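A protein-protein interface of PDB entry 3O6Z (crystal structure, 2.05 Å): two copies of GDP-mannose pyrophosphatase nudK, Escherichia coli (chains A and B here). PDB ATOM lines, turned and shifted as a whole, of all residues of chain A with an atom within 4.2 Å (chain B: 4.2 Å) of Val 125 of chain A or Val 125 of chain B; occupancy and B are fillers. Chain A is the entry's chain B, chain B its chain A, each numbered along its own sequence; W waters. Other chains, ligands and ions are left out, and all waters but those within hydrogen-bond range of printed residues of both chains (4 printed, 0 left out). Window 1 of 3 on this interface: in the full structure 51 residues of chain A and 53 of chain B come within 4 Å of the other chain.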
ATOM      1  N   TYR A  42      15.115 -34.250  19.276  1.00  0.00           N
ATOM      2  CA  TYR A  42      15.051 -33.798  20.662  1.00  0.00           C
ATOM      3  C   TYR A  42      13.592 -33.496  20.969  1.00  0.00           C
ATOM      4  O   TYR A  42      12.962 -32.643  20.308  1.00  0.00           O
ATOM      5  CB  TYR A  42      15.921 -32.549  20.863  1.00  0.00           C
ATOM      6  CG  TYR A  42      16.092 -32.064  22.299  1.00  0.00           C
ATOM      7  CD1 TYR A  42      16.169 -32.968  23.373  1.00  0.00           C
ATOM      8  CD2 TYR A  42      16.233 -30.695  22.571  1.00  0.00           C
ATOM      9  CE1 TYR A  42      16.354 -32.522  24.690  1.00  0.00           C
ATOM     10  CE2 TYR A  42      16.447 -30.231  23.898  1.00  0.00           C
ATOM     11  CZ  TYR A  42      16.488 -31.149  24.943  1.00  0.00           C
ATOM     12  OH  TYR A  42      16.653 -30.700  26.234  1.00  0.00           O
ATOM     13  N   ALA A  69      20.552 -21.201  26.745  1.00  0.00           N
ATOM     14  CA  ALA A  69      20.706 -21.648  25.368  1.00  0.00           C
ATOM     15  C   ALA A  69      21.058 -20.513  24.399  1.00  0.00           C
ATOM     16  O   ALA A  69      21.775 -20.739  23.438  1.00  0.00           O
ATOM     17  CB  ALA A  69      19.424 -22.365  24.905  1.00  0.00           C
ATOM     18  N   SER A 121      11.237 -25.735  15.170  1.00  0.00           N
ATOM     19  CA  SER A 121      12.595 -26.142  14.781  1.00  0.00           C
ATOM     20  C   SER A 121      12.596 -27.585  14.297  1.00  0.00           C
ATOM     21  O   SER A 121      13.109 -28.474  14.976  1.00  0.00           O
ATOM     22  CB  SER A 121      13.558 -25.960  15.953  1.00  0.00           C
ATOM     23  OG  SER A 121      14.885 -26.086  15.472  1.00  0.00           O
ATOM     24  N   PRO A 122      11.983 -27.834  13.129  1.00  0.00           N
ATOM     25  CA  PRO A 122      11.658 -29.205  12.736  1.00  0.00           C
ATOM     26  C   PRO A 122      12.797 -30.045  12.158  1.00  0.00           C
ATOM     27  O   PRO A 122      12.563 -31.195  11.817  1.00  0.00           O
ATOM     28  CB  PRO A 122      10.543 -28.998  11.692  1.00  0.00           C
ATOM     29  CG  PRO A 122      10.929 -27.736  11.017  1.00  0.00           C
ATOM     30  CD  PRO A 122      11.429 -26.850  12.178  1.00  0.00           C
ATOM     31  N   GLY A 123      13.995 -29.456  12.056  1.00  0.00           N
ATOM     32  CA  GLY A 123      15.202 -30.149  11.629  1.00  0.00           C
ATOM     33  C   GLY A 123      15.477 -31.247  12.631  1.00  0.00           C
ATOM     34  O   GLY A 123      15.643 -32.362  12.234  1.00  0.00           O
ATOM     35  N   GLY A 124      15.504 -30.950  13.925  1.00  0.00           N
ATOM     36  CA  GLY A 124      15.703 -32.028  14.909  1.00  0.00           C
ATOM     37  C   GLY A 124      15.025 -31.843  16.266  1.00  0.00           C
ATOM     38  O   GLY A 124      15.431 -32.446  17.254  1.00  0.00           O
ATOM     39  N   VAL A 125      13.985 -31.017  16.320  1.00  0.00           N
ATOM     40  CA  VAL A 125      13.260 -30.796  17.588  1.00  0.00           C
ATOM     41  C   VAL A 125      11.783 -31.015  17.265  1.00  0.00           C
ATOM     42  O   VAL A 125      11.306 -30.590  16.225  1.00  0.00           O
ATOM     43  CB  VAL A 125      13.554 -29.352  18.174  1.00  0.00           C
ATOM     44  CG1 VAL A 125      12.949 -29.147  19.589  1.00  0.00           C
ATOM     45  CG2 VAL A 125      15.044 -29.063  18.215  1.00  0.00           C
ATOM     46  N   THR A 126      11.059 -31.683  18.156  1.00  0.00           N
ATOM     47  CA  THR A 126       9.659 -32.001  17.921  1.00  0.00           C
ATOM     48  C   THR A 126       8.716 -30.801  18.095  1.00  0.00           C
ATOM     49  O   THR A 126       7.594 -30.792  17.554  1.00  0.00           O
ATOM     50  CB  THR A 126       9.165 -33.100  18.887  1.00  0.00           C
ATOM     51  OG1 THR A 126       9.361 -32.665  20.225  1.00  0.00           O
ATOM     52  CG2 THR A 126       9.913 -34.421  18.656  1.00  0.00           C
ATOM     53  N   GLU A 127       9.193 -29.809  18.851  1.00  0.00           N
ATOM     54  CA  GLU A 127       8.376 -28.771  19.439  1.00  0.00           C
ATOM     55  C   GLU A 127       7.361 -28.167  18.502  1.00  0.00           C
ATOM     56  O   GLU A 127       7.731 -27.640  17.442  1.00  0.00           O
ATOM     57  CB  GLU A 127       9.263 -27.660  19.984  1.00  0.00           C
ATOM     58  CG  GLU A 127       8.489 -26.545  20.610  1.00  0.00           C
ATOM     59  CD  GLU A 127       9.396 -25.466  21.108  1.00  0.00           C
ATOM     60  OE1 GLU A 127       9.947 -24.704  20.286  1.00  0.00           O
ATOM     61  OE2 GLU A 127       9.571 -25.420  22.322  1.00  0.00           O
ATOM     62  N   TYR B  42      20.493 -28.044  23.967  1.00  0.00           N
ATOM     63  CA  TYR B  42      20.789 -28.824  22.789  1.00  0.00           C
ATOM     64  C   TYR B  42      21.392 -27.912  21.755  1.00  0.00           C
ATOM     65  O   TYR B  42      20.745 -26.977  21.305  1.00  0.00           O
ATOM     66  CB  TYR B  42      19.513 -29.507  22.273  1.00  0.00           C
ATOM     67  CG  TYR B  42      19.731 -30.520  21.170  1.00  0.00           C
ATOM     68  CD1 TYR B  42      20.865 -31.339  21.145  1.00  0.00           C
ATOM     69  CD2 TYR B  42      18.780 -30.674  20.150  1.00  0.00           C
ATOM     70  CE1 TYR B  42      21.052 -32.268  20.122  1.00  0.00           C
ATOM     71  CE2 TYR B  42      18.964 -31.616  19.139  1.00  0.00           C
ATOM     72  CZ  TYR B  42      20.092 -32.399  19.143  1.00  0.00           C
ATOM     73  OH  TYR B  42      20.270 -33.324  18.144  1.00  0.00           O
ATOM     74  N   ALA B  69      11.240 -35.385  13.010  1.00  0.00           N
ATOM     75  CA  ALA B  69      10.917 -34.786  14.312  1.00  0.00           C
ATOM     76  C   ALA B  69       9.443 -34.395  14.423  1.00  0.00           C
ATOM     77  O   ALA B  69       8.858 -34.324  15.507  1.00  0.00           O
ATOM     78  CB  ALA B  69      11.820 -33.600  14.568  1.00  0.00           C
ATOM     79  N   SER B 121      13.789 -21.611  19.166  1.00  0.00           N
ATOM     80  CA  SER B 121      13.323 -22.449  20.309  1.00  0.00           C
ATOM     81  C   SER B 121      14.238 -22.282  21.519  1.00  0.00           C
ATOM     82  O   SER B 121      14.975 -23.218  21.870  1.00  0.00           O
ATOM     83  CB  SER B 121      13.287 -23.928  19.876  1.00  0.00           C
ATOM     84  OG  SER B 121      12.695 -24.762  20.858  1.00  0.00           O
ATOM     85  N   PRO B 122      14.214 -21.081  22.150  1.00  0.00           N
ATOM     86  CA  PRO B 122      15.230 -20.722  23.174  1.00  0.00           C
ATOM     87  C   PRO B 122      15.106 -21.397  24.537  1.00  0.00           C
ATOM     88  O   PRO B 122      16.011 -21.252  25.377  1.00  0.00           O
ATOM     89  CB  PRO B 122      15.070 -19.179  23.316  1.00  0.00           C
ATOM     90  CG  PRO B 122      13.626 -18.928  22.969  1.00  0.00           C
ATOM     91  CD  PRO B 122      13.290 -19.961  21.877  1.00  0.00           C
ATOM     92  N   GLY B 123      13.990 -22.080  24.777  1.00  0.00           N
ATOM     93  CA  GLY B 123      13.770 -22.874  26.012  1.00  0.00           C
ATOM     94  C   GLY B 123      14.899 -23.846  26.238  1.00  0.00           C
ATOM     95  O   GLY B 123      15.459 -23.920  27.341  1.00  0.00           O
ATOM     96  N   GLY B 124      15.275 -24.569  25.177  1.00  0.00           N
ATOM     97  CA  GLY B 124      16.280 -25.612  25.309  1.00  0.00           C
ATOM     98  C   GLY B 124      17.205 -25.845  24.122  1.00  0.00           C
ATOM     99  O   GLY B 124      18.036 -26.740  24.164  1.00  0.00           O
ATOM    100  N   VAL B 125      17.099 -24.993  23.100  1.00  0.00           N
ATOM    101  CA  VAL B 125      17.843 -25.165  21.849  1.00  0.00           C
ATOM    102  C   VAL B 125      18.563 -23.871  21.507  1.00  0.00           C
ATOM    103  O   VAL B 125      17.964 -22.806  21.558  1.00  0.00           O
ATOM    104  CB  VAL B 125      16.871 -25.581  20.683  1.00  0.00           C
ATOM    105  CG1 VAL B 125      17.659 -25.949  19.416  1.00  0.00           C
ATOM    106  CG2 VAL B 125      15.989 -26.736  21.149  1.00  0.00           C
ATOM    107  N   THR B 126      19.836 -23.973  21.139  1.00  0.00           N
ATOM    108  CA  THR B 126      20.681 -22.806  20.844  1.00  0.00           C
ATOM    109  C   THR B 126      20.287 -22.115  19.556  1.00  0.00           C
ATOM    110  O   THR B 126      20.613 -20.950  19.357  1.00  0.00           O
ATOM    111  CB  THR B 126      22.199 -23.166  20.703  1.00  0.00           C
ATOM    112  OG1 THR B 126      22.426 -24.009  19.552  1.00  0.00           O
ATOM    113  CG2 THR B 126      22.737 -23.840  21.950  1.00  0.00           C
ATOM    114  N   GLU B 127      19.596 -22.850  18.688  1.00  0.00           N
ATOM    115  CA  GLU B 127      19.489 -22.502  17.273  1.00  0.00           C
ATOM    116  C   GLU B 127      19.085 -21.048  16.986  1.00  0.00           C
ATOM    117  O   GLU B 127      18.009 -20.591  17.425  1.00  0.00           O
ATOM    118  CB  GLU B 127      18.507 -23.454  16.589  1.00  0.00           C
ATOM    119  CG  GLU B 127      18.189 -23.070  15.135  1.00  0.00           C
ATOM    120  CD  GLU B 127      17.118 -23.944  14.524  1.00  0.00           C
ATOM    121  OE1 GLU B 127      15.920 -23.733  14.812  1.00  0.00           O
ATOM    122  OE2 GLU B 127      17.471 -24.844  13.737  1.00  0.00           O
HETATM  123  O   HOH W   1      15.465 -26.737  11.770  1.00  0.00           O
HETATM  124  O   HOH W   2      17.643 -21.453  27.547  1.00  0.00           O
HETATM  125  O   HOH W   3      13.050 -33.870  11.355  1.00  0.00           O
HETATM  126  O   HOH W   4      11.224 -23.166  23.544  1.00  0.00           O
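OG of Ser 121 of chain A is in hydrogen-bond range of OE1 of Glu 127 of chain B, 2.7 Å away. The side-chain hydroxyl (OG) of Ser 121 of chain B lies within hydrogen-bond range of the side-chain carboxylate (OE1) of Glu 127 of chain A (2.8 Å).
N of Tyr 42 of chain A is in hydrogen-bond range of O of Gly 124 of chain A (2.7 Å). The backbone carbonyl oxygen (O) of Tyr 42 of chain B is in hydrogen-bond range of the backbone NH (N) of Thr 126 of chain B (3.1 Å). N of Tyr 42 of chain B lies within hydrogen-bond range of O of Gly 124 of chain B, at 2.8 Å. The backbone carbonyl oxygen (O) of Tyr 42 of chain A lies within hydrogen-bond range of the backbone NH (N) of Thr 126 of chain A (3.0 Å).
Among the printed residues, merely in contact across the chains: Tyr 42 of chain A with Tyr 42 of chain B (3.5 Å), Tyr 42 of chain A with Gly 124 of chain B (3.8 Å), Ala 69 of chain A with Pro 122 of chain B (3.6 Å), Ala 69 of chain A with Val 125 of chain B (3.7 Å), Ala 69 of chain A with Thr 126 of chain B (3.5 Å), Pro 122 of chain A with Ala 69 of chain B (3.7 Å), Val 125 of chain A with Ala 69 of chain B (3.5 Å), Val 125 of chain A with Val 125 of chain B (3.9 Å) and Thr 126 of chain A with Ala 69 of chain B (3.3 Å).
Of the printed residues of chain A, Val 125 of chain B touches Ala 69 and Val 125. Printed residues of chain A within 4 Å of Gly 124 of chain B: Tyr 42. Of the printed residues of chain A, Pro 122 of chain B touches Ala 69. Of the printed residues of chain A, Thr 126 of chain B touches Ala 69. Printed residues of chain A within 4 Å of Ala 69 of chain B: Pro 122, Val 125 and Thr 126. Of the printed residues of chain B, Ser 121 of chain A touches Glu 127. The nearest printed residue of chain B that does not touch Ala 69 of chain A is Gly 124 of chain B (4.2 Å).
Of the 9 printed residues of chain A, 7 touch a printed residue of chain B. Of the 9 printed residues of chain B, 8 touch a printed residue of chain A. Hydrophobic or aromatic side chains of chain B within 4 Å of the printed part of chain A: Tyr 42, Ala 69 and Val 125. Among the printed residues, no Asp or Glu carboxylate lies within 4 Å of a Lys or Arg side-chain nitrogen of the other chain.
Tyr 42 of chain A touches Gly 124 of chain B, but with the chains exchanged Gly 124 of chain A does not touch Tyr 42 of chain B (4.1 Å). Ala 69 of chain A touches Pro 122 of chain B, and with the chains exchanged Pro 122 of chain A touches Ala 69 of chain B. Ala 69 of chain A touches Val 125 of chain B, and with the chains exchanged Val 125 of chain A touches Ala 69 of chain B. Val 125 of chain B touches its own counterpart, Val 125 of chain A. Positions printed for both chains: 42, 69, 121, 122, 123, 124, 125, 126 and 127.
Water W2 lies within hydrogen-bond range of the backbone carbonyl oxygen (O) of Pro 122 of chain B (2.7 Å), the backbone NH (N) of Ala 69 of chain A (3.0 Å) and the backbone carbonyl oxygen (O) of Gly 123 of chain B (3.3 Å). Water W3 lies within hydrogen-bond range of O of Pro 122 of chain A (2.8 Å), N of Ala 69 of chain B (2.9 Å) and O of Gly 123 of chain A (3.1 Å). Water W4 lies within hydrogen-bond range of the side-chain carboxylate (OE2) of Glu 127 of chain A (3.1 Å), the backbone NH (N) of Gly 123 of chain B (3.2 Å) and the side-chain hydroxyl (OG) of Ser 121 of chain B (3.5 Å). Water W1 bridges N of Gly 123 of chain A and OE2 of Glu 127 of chain B.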
